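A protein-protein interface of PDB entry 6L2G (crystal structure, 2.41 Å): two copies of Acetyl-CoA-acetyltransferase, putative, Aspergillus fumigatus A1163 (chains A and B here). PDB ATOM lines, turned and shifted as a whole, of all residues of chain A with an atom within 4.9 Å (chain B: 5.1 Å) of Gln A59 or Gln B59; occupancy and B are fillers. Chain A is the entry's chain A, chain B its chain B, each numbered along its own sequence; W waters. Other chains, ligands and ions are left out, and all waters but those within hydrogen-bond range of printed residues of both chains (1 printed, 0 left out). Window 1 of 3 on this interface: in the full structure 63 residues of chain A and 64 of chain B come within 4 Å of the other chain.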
ATOM      1  N   ASN A  56       3.822  28.521 -15.000  1.00  0.00           N
ATOM      2  CA  ASN A  56       4.096  29.676 -15.879  1.00  0.00           C
ATOM      3  C   ASN A  56       2.809  30.022 -16.628  1.00  0.00           C
ATOM      4  O   ASN A  56       2.390  29.216 -17.484  1.00  0.00           O
ATOM      5  CB  ASN A  56       5.251  29.341 -16.829  1.00  0.00           C
ATOM      6  CG  ASN A  56       5.670  30.510 -17.697  1.00  0.00           C
ATOM      7  OD1 ASN A  56       5.931  30.326 -18.884  1.00  0.00           O
ATOM      8  ND2 ASN A  56       5.726  31.702 -17.119  1.00  0.00           N
ATOM      9  N   VAL A  57       2.177  31.153 -16.324  1.00  0.00           N
ATOM     10  CA  VAL A  57       0.803  31.388 -16.860  1.00  0.00           C
ATOM     11  C   VAL A  57       0.878  32.106 -18.212  1.00  0.00           C
ATOM     12  O   VAL A  57       0.046  31.817 -19.043  1.00  0.00           O
ATOM     13  CB  VAL A  57      -0.192  32.013 -15.842  1.00  0.00           C
ATOM     14  CG1 VAL A  57       0.358  32.166 -14.440  1.00  0.00           C
ATOM     15  CG2 VAL A  57      -0.833  33.295 -16.323  1.00  0.00           C
ATOM     16  N   LEU A  58       1.832  32.997 -18.420  1.00  0.00           N
ATOM     17  CA  LEU A  58       1.936  33.820 -19.641  1.00  0.00           C
ATOM     18  C   LEU A  58       3.215  33.389 -20.386  1.00  0.00           C
ATOM     19  O   LEU A  58       4.285  34.026 -20.187  1.00  0.00           O
ATOM     20  CB  LEU A  58       1.931  35.293 -19.220  1.00  0.00           C
ATOM     21  CG  LEU A  58       0.690  35.729 -18.432  1.00  0.00           C
ATOM     22  CD1 LEU A  58       0.783  37.174 -17.925  1.00  0.00           C
ATOM     23  CD2 LEU A  58      -0.571  35.531 -19.269  1.00  0.00           C
ATOM     24  N   GLN A  59       3.071  32.362 -21.236  1.00  0.00           N
ATOM     25  CA  GLN A  59       4.138  31.628 -21.968  1.00  0.00           C
ATOM     26  C   GLN A  59       4.543  32.341 -23.267  1.00  0.00           C
ATOM     27  O   GLN A  59       5.586  31.970 -23.836  1.00  0.00           O
ATOM     28  CB  GLN A  59       3.645  30.206 -22.214  1.00  0.00           C
ATOM     29  CG  GLN A  59       3.554  29.444 -20.902  1.00  0.00           C
ATOM     30  CD  GLN A  59       2.763  28.172 -21.000  1.00  0.00           C
ATOM     31  OE1 GLN A  59       2.582  27.633 -22.087  1.00  0.00           O
ATOM     32  NE2 GLN A  59       2.296  27.698 -19.852  1.00  0.00           N
ATOM     33  N   GLY A  60       3.818  33.377 -23.676  1.00  0.00           N
ATOM     34  CA  GLY A  60       4.076  34.093 -24.942  1.00  0.00           C
ATOM     35  C   GLY A  60       5.502  34.617 -25.014  1.00  0.00           C
ATOM     36  O   GLY A  60       5.903  35.368 -24.087  1.00  0.00           O
ATOM     37  N   ALA A  61       6.235  34.222 -26.068  1.00  0.00           N
ATOM     38  CA  ALA A  61       7.608  34.678 -26.408  1.00  0.00           C
ATOM     39  C   ALA A  61       8.606  34.195 -25.348  1.00  0.00           C
ATOM     40  O   ALA A  61       9.737  34.650 -25.378  1.00  0.00           O
ATOM     41  CB  ALA A  61       7.683  36.186 -26.581  1.00  0.00           C
ATOM     42  N   VAL A  62       8.247  33.234 -24.505  1.00  0.00           N
ATOM     43  CA  VAL A  62       9.218  32.637 -23.539  1.00  0.00           C
ATOM     44  C   VAL A  62      10.092  31.624 -24.288  1.00  0.00           C
ATOM     45  O   VAL A  62      11.206  31.259 -23.789  1.00  0.00           O
ATOM     46  CB  VAL A  62       8.478  32.008 -22.348  1.00  0.00           C
ATOM     47  CG1 VAL A  62       9.454  31.350 -21.392  1.00  0.00           C
ATOM     48  CG2 VAL A  62       7.632  33.038 -21.610  1.00  0.00           C
ATOM     49  N   GLY A  63       9.609  31.189 -25.454  1.00  0.00           N
ATOM     50  CA  GLY A  63      10.312  30.221 -26.303  1.00  0.00           C
ATOM     51  C   GLY A  63       9.846  28.829 -25.961  1.00  0.00           C
ATOM     52  O   GLY A  63       9.057  28.686 -25.020  1.00  0.00           O
ATOM     53  N   PRO A  66       9.091  26.207 -21.777  1.00  0.00           N
ATOM     54  CA  PRO A  66       9.648  27.048 -20.726  1.00  0.00           C
ATOM     55  C   PRO A  66      10.259  26.268 -19.552  1.00  0.00           C
ATOM     56  O   PRO A  66      11.342  26.655 -19.116  1.00  0.00           O
ATOM     57  CB  PRO A  66       8.451  27.902 -20.287  1.00  0.00           C
ATOM     58  CG  PRO A  66       7.612  28.035 -21.542  1.00  0.00           C
ATOM     59  CD  PRO A  66       7.785  26.700 -22.245  1.00  0.00           C
ATOM     60  N   THR A  84       5.597  22.335 -18.357  1.00  0.00           N
ATOM     61  CA  THR A  84       5.206  23.659 -17.835  1.00  0.00           C
ATOM     62  C   THR A  84       3.688  23.648 -17.635  1.00  0.00           C
ATOM     63  O   THR A  84       2.977  23.197 -18.547  1.00  0.00           O
ATOM     64  CB  THR A  84       5.835  24.785 -18.662  1.00  0.00           C
ATOM     65  OG1 THR A  84       4.791  25.697 -18.994  1.00  0.00           O
ATOM     66  CG2 THR A  84       6.577  24.300 -19.883  1.00  0.00           C
ATOM     67  N   VAL A  85       3.239  24.093 -16.456  1.00  0.00           N
ATOM     68  CA  VAL A  85       1.836  23.943 -15.982  1.00  0.00           C
ATOM     69  C   VAL A  85       1.170  25.330 -15.897  1.00  0.00           C
ATOM     70  O   VAL A  85       1.836  26.313 -15.564  1.00  0.00           O
ATOM     71  CB  VAL A  85       1.748  23.063 -14.714  1.00  0.00           C
ATOM     72  CG1 VAL A  85       3.099  22.684 -14.137  1.00  0.00           C
ATOM     73  CG2 VAL A  85       0.831  23.607 -13.628  1.00  0.00           C
ATOM     74  N   ASN A  86      -0.092  25.410 -16.335  1.00  0.00           N
ATOM     75  CA  ASN A  86      -0.929  26.636 -16.334  1.00  0.00           C
ATOM     76  C   ASN A  86      -2.253  26.321 -15.618  1.00  0.00           C
ATOM     77  O   ASN A  86      -3.192  25.792 -16.245  1.00  0.00           O
ATOM     78  CB  ASN A  86      -1.114  27.204 -17.747  1.00  0.00           C
ATOM     79  CG  ASN A  86      -1.944  28.473 -17.787  1.00  0.00           C
ATOM     80  OD1 ASN A  86      -2.406  28.963 -16.747  1.00  0.00           O
ATOM     81  ND2 ASN A  86      -2.139  29.014 -18.984  1.00  0.00           N
ATOM     82  N   ASP A 147      -4.836  37.331 -21.325  1.00  0.00           N
ATOM     83  CA  ASP A 147      -4.544  35.943 -20.862  1.00  0.00           C
ATOM     84  C   ASP A 147      -4.398  35.903 -19.332  1.00  0.00           C
ATOM     85  O   ASP A 147      -4.623  34.838 -18.739  1.00  0.00           O
ATOM     86  CB  ASP A 147      -3.282  35.396 -21.537  1.00  0.00           C
ATOM     87  CG  ASP A 147      -3.428  35.180 -23.039  1.00  0.00           C
ATOM     88  OD1 ASP A 147      -4.555  35.365 -23.543  1.00  0.00           O
ATOM     89  OD2 ASP A 147      -2.409  34.798 -23.698  1.00  0.00           O
ATOM     90  N   ASN B  56      -2.240  22.269 -24.588  1.00  0.00           N
ATOM     91  CA  ASN B  56      -2.313  23.473 -25.439  1.00  0.00           C
ATOM     92  C   ASN B  56      -0.904  24.058 -25.448  1.00  0.00           C
ATOM     93  O   ASN B  56      -0.404  24.337 -24.365  1.00  0.00           O
ATOM     94  CB  ASN B  56      -3.381  24.433 -24.901  1.00  0.00           C
ATOM     95  CG  ASN B  56      -3.608  25.639 -25.784  1.00  0.00           C
ATOM     96  OD1 ASN B  56      -3.674  26.755 -25.297  1.00  0.00           O
ATOM     97  ND2 ASN B  56      -3.745  25.426 -27.077  1.00  0.00           N
ATOM     98  N   VAL B  57      -0.256  24.161 -26.602  1.00  0.00           N
ATOM     99  CA  VAL B  57       1.194  24.515 -26.646  1.00  0.00           C
ATOM    100  C   VAL B  57       1.369  26.033 -26.763  1.00  0.00           C
ATOM    101  O   VAL B  57       2.228  26.582 -26.078  1.00  0.00           O
ATOM    102  CB  VAL B  57       1.921  23.790 -27.785  1.00  0.00           C
ATOM    103  CG1 VAL B  57       3.359  24.259 -27.827  1.00  0.00           C
ATOM    104  CG2 VAL B  57       1.853  22.285 -27.636  1.00  0.00           C
ATOM    105  N   LEU B  58       0.618  26.650 -27.665  1.00  0.00           N
ATOM    106  CA  LEU B  58       0.674  28.083 -28.007  1.00  0.00           C
ATOM    107  C   LEU B  58      -0.581  28.764 -27.439  1.00  0.00           C
ATOM    108  O   LEU B  58      -1.621  28.824 -28.123  1.00  0.00           O
ATOM    109  CB  LEU B  58       0.805  28.150 -29.523  1.00  0.00           C
ATOM    110  CG  LEU B  58       1.939  27.276 -30.047  1.00  0.00           C
ATOM    111  CD1 LEU B  58       1.942  27.205 -31.560  1.00  0.00           C
ATOM    112  CD2 LEU B  58       3.278  27.782 -29.539  1.00  0.00           C
ATOM    113  N   GLN B  59      -0.452  29.253 -26.201  1.00  0.00           N
ATOM    114  CA  GLN B  59      -1.550  29.754 -25.341  1.00  0.00           C
ATOM    115  C   GLN B  59      -1.794  31.233 -25.611  1.00  0.00           C
ATOM    116  O   GLN B  59      -2.804  31.745 -25.137  1.00  0.00           O
ATOM    117  CB  GLN B  59      -1.199  29.475 -23.877  1.00  0.00           C
ATOM    118  CG  GLN B  59      -1.338  27.991 -23.552  1.00  0.00           C
ATOM    119  CD  GLN B  59      -0.774  27.523 -22.230  1.00  0.00           C
ATOM    120  OE1 GLN B  59      -0.629  28.278 -21.277  1.00  0.00           O
ATOM    121  NE2 GLN B  59      -0.494  26.236 -22.149  1.00  0.00           N
ATOM    122  N   GLY B  60      -0.920  31.901 -26.355  1.00  0.00           N
ATOM    123  CA  GLY B  60      -1.016  33.362 -26.561  1.00  0.00           C
ATOM    124  C   GLY B  60      -2.346  33.761 -27.183  1.00  0.00           C
ATOM    125  O   GLY B  60      -2.722  33.173 -28.216  1.00  0.00           O
ATOM    126  N   ALA B  61      -3.030  34.719 -26.560  1.00  0.00           N
ATOM    127  CA  ALA B  61      -4.247  35.409 -27.040  1.00  0.00           C
ATOM    128  C   ALA B  61      -5.446  34.459 -27.009  1.00  0.00           C
ATOM    129  O   ALA B  61      -6.495  34.823 -27.570  1.00  0.00           O
ATOM    130  CB  ALA B  61      -4.006  35.970 -28.420  1.00  0.00           C
ATOM    131  N   VAL B  62      -5.305  33.312 -26.342  1.00  0.00           N
ATOM    132  CA  VAL B  62      -6.378  32.295 -26.164  1.00  0.00           C
ATOM    133  C   VAL B  62      -7.290  32.734 -25.011  1.00  0.00           C
ATOM    134  O   VAL B  62      -8.387  32.180 -24.856  1.00  0.00           O
ATOM    135  CB  VAL B  62      -5.746  30.910 -25.933  1.00  0.00           C
ATOM    136  CG1 VAL B  62      -6.778  29.838 -25.644  1.00  0.00           C
ATOM    137  CG2 VAL B  62      -4.910  30.497 -27.130  1.00  0.00           C
ATOM    138  N   GLY B  63      -6.850  33.716 -24.229  1.00  0.00           N
ATOM    139  CA  GLY B  63      -7.561  34.186 -23.031  1.00  0.00           C
ATOM    140  C   GLY B  63      -7.225  33.341 -21.826  1.00  0.00           C
ATOM    141  O   GLY B  63      -6.510  32.325 -21.972  1.00  0.00           O
ATOM    142  N   PRO B  66      -7.114  28.338 -20.780  1.00  0.00           N
ATOM    143  CA  PRO B  66      -7.648  27.613 -21.935  1.00  0.00           C
ATOM    144  C   PRO B  66      -8.446  26.354 -21.577  1.00  0.00           C
ATOM    145  O   PRO B  66      -9.521  26.232 -22.077  1.00  0.00           O
ATOM    146  CB  PRO B  66      -6.398  27.260 -22.746  1.00  0.00           C
ATOM    147  CG  PRO B  66      -5.440  28.420 -22.450  1.00  0.00           C
ATOM    148  CD  PRO B  66      -5.753  28.844 -21.023  1.00  0.00           C
ATOM    149  N   THR B  84      -4.363  23.649 -17.931  1.00  0.00           N
ATOM    150  CA  THR B  84      -3.796  23.674 -19.305  1.00  0.00           C
ATOM    151  C   THR B  84      -2.360  23.136 -19.194  1.00  0.00           C
ATOM    152  O   THR B  84      -1.606  23.656 -18.345  1.00  0.00           O
ATOM    153  CB  THR B  84      -3.968  25.078 -19.906  1.00  0.00           C
ATOM    154  OG1 THR B  84      -5.297  25.505 -19.592  1.00  0.00           O
ATOM    155  CG2 THR B  84      -3.786  25.121 -21.405  1.00  0.00           C
ATOM    156  N   VAL B  85      -2.020  22.093 -19.955  1.00  0.00           N
ATOM    157  CA  VAL B  85      -0.714  21.385 -19.838  1.00  0.00           C
ATOM    158  C   VAL B  85       0.127  21.627 -21.100  1.00  0.00           C
ATOM    159  O   VAL B  85      -0.424  21.631 -22.218  1.00  0.00           O
ATOM    160  CB  VAL B  85      -0.899  19.904 -19.439  1.00  0.00           C
ATOM    161  CG1 VAL B  85      -2.346  19.491 -19.333  1.00  0.00           C
ATOM    162  CG2 VAL B  85      -0.091  18.917 -20.266  1.00  0.00           C
ATOM    163  N   ASN B  86       1.426  21.890 -20.904  1.00  0.00           N
ATOM    164  CA  ASN B  86       2.379  22.180 -22.002  1.00  0.00           C
ATOM    165  C   ASN B  86       3.604  21.263 -21.871  1.00  0.00           C
ATOM    166  O   ASN B  86       4.588  21.616 -21.179  1.00  0.00           O
ATOM    167  CB  ASN B  86       2.709  23.661 -22.079  1.00  0.00           C
ATOM    168  CG  ASN B  86       3.592  24.004 -23.257  1.00  0.00           C
ATOM    169  OD1 ASN B  86       3.980  23.111 -24.031  1.00  0.00           O
ATOM    170  ND2 ASN B  86       3.948  25.282 -23.367  1.00  0.00           N
ATOM    171  N   ASP B 147       7.878  30.052 -30.145  1.00  0.00           N
ATOM    172  CA  ASP B 147       7.374  29.199 -29.028  1.00  0.00           C
ATOM    173  C   ASP B 147       7.158  27.744 -29.492  1.00  0.00           C
ATOM    174  O   ASP B 147       7.369  26.830 -28.676  1.00  0.00           O
ATOM    175  CB  ASP B 147       6.134  29.828 -28.375  1.00  0.00           C
ATOM    176  CG  ASP B 147       6.434  31.144 -27.664  1.00  0.00           C
ATOM    177  OD1 ASP B 147       7.614  31.386 -27.355  1.00  0.00           O
ATOM    178  OD2 ASP B 147       5.486  31.941 -27.417  1.00  0.00           O
HETATM  179  O   HOH W   1       1.926  28.704 -24.557  1.00  0.00           O
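NE2 of Gln A59 sits at hydrogen-bond distance from OE1 of Gln B59, at 3.3 Å.
The side-chain amide oxygen (OE1) of Gln A59 is in hydrogen-bond range of the side-chain amide nitrogen (ND2) of Asn B86 (3.0 Å).
N of Ala A61 is in hydrogen-bond range of OD2 of Asp B147, 2.8 Å away.
N of Val A62 lies within hydrogen-bond range of OD1 of Asp B147.
The backbone NH of Gly A63 is in hydrogen-bond range of the side-chain carboxylate of Asp B147 (2.8 Å).
The backbone NH (N) of Thr A84 is in hydrogen-bond range of the backbone carbonyl oxygen (O) of Asn B86, at 3.1 Å.
ND2 of Asn A86 is in hydrogen-bond range of OE1 of Gln B59, at 2.8 Å.
The backbone NH (N) of Thr B84 is in hydrogen-bond range of the backbone carbonyl oxygen (O) of Asn A86, 3.0 Å away.
The side-chain carboxylate (OD2) of Asp A147 is in hydrogen-bond range of the backbone NH (N) of Ala B61 (2.9 Å).
N of Gly B63 is in hydrogen-bond range of OD1 of Asp A147, at 2.9 Å.
OD2 of Asp A147 lies close to O of Gln B59 (3.4 Å).
Gln A59 touches its own counterpart, Gln B59.
Gln A59 touches Asp B147, and with the chains exchanged Asp A147 touches Gln B59.
Ala A61 touches Asp B147, and with the chains exchanged Asp A147 touches Ala B61.
Thr A84 touches Asn B86, and with the chains exchanged Asn A86 touches Thr B84.
Water W1 lies within hydrogen-bond range of the backbone carbonyl oxygen (O) of Val B57 (2.6 Å), the side-chain amide oxygen (OE1) of Gln A59 (2.8 Å) and the backbone NH (N) of Gln B59 (2.9 Å).
Gln A59 touches three residues of chain B.
Of chain A, only Gln A59 (3.3 Å), Asn A86 (2.8 Å) and Asp A147 (3.4 Å) come within 4 Å of Gln B59.
Of the printed residues of chain A, Gly B63 touches Asp A147 (2.9 Å).
Of the printed residues of chain A, Asp B147 touches Gln A59 (3.6 Å), Gly A60 (3.6 Å), Ala A61 (2.8 Å), Val A62 (3.5 Å) and Gly A63 (2.8 Å).
Val B85 touches none of the printed residues of chain A.
Val B57 touches none of the printed residues of chain A.
The nearest residue of chain B that does not touch Gln A59 is Val B57 (4.1 Å).
Of the 13 printed residues of chain B, 8 touch a printed residue of chain A.
Along chain B the printed residues that touch a printed residue of chain A span positions 59 to 147.
Printed residues of chain A that touch a printed residue of chain B: Gln A59, Gly A60, Ala A61, Val A62, Gly A63, Thr A84, Asn A86 and Asp A147.
Among the printed residues, 15 pairs touch across the chains.
Among the printed residues, no Asp or Glu carboxylate lies within 4 Å of a Lys or Arg side-chain nitrogen of the other chain.
The backbone carbonyl oxygen of Asn A56 is in hydrogen-bond range of the side-chain amide nitrogen of Gln A59 (2.8 Å).
OG1 of Thr A84 is in hydrogen-bond range of NE2 of Gln A59, 3.3 Å away.
NE2 of Gln B59 sits at hydrogen-bond distance from O of Asn B56.
The side-chain amide nitrogen (ND2) of Asn B86 lies within hydrogen-bond range of the backbone carbonyl oxygen (O) of Val B57 (3.5 Å).
Among the printed residues, merely in contact across the chains: Asp A147 with Gly B60 (3.5 Å), Asp A147 with Val B62 (3.6 Å), Gly A60 with Asp B147 (3.6 Å) and Gln A59 with Asp B147 (3.6 Å).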
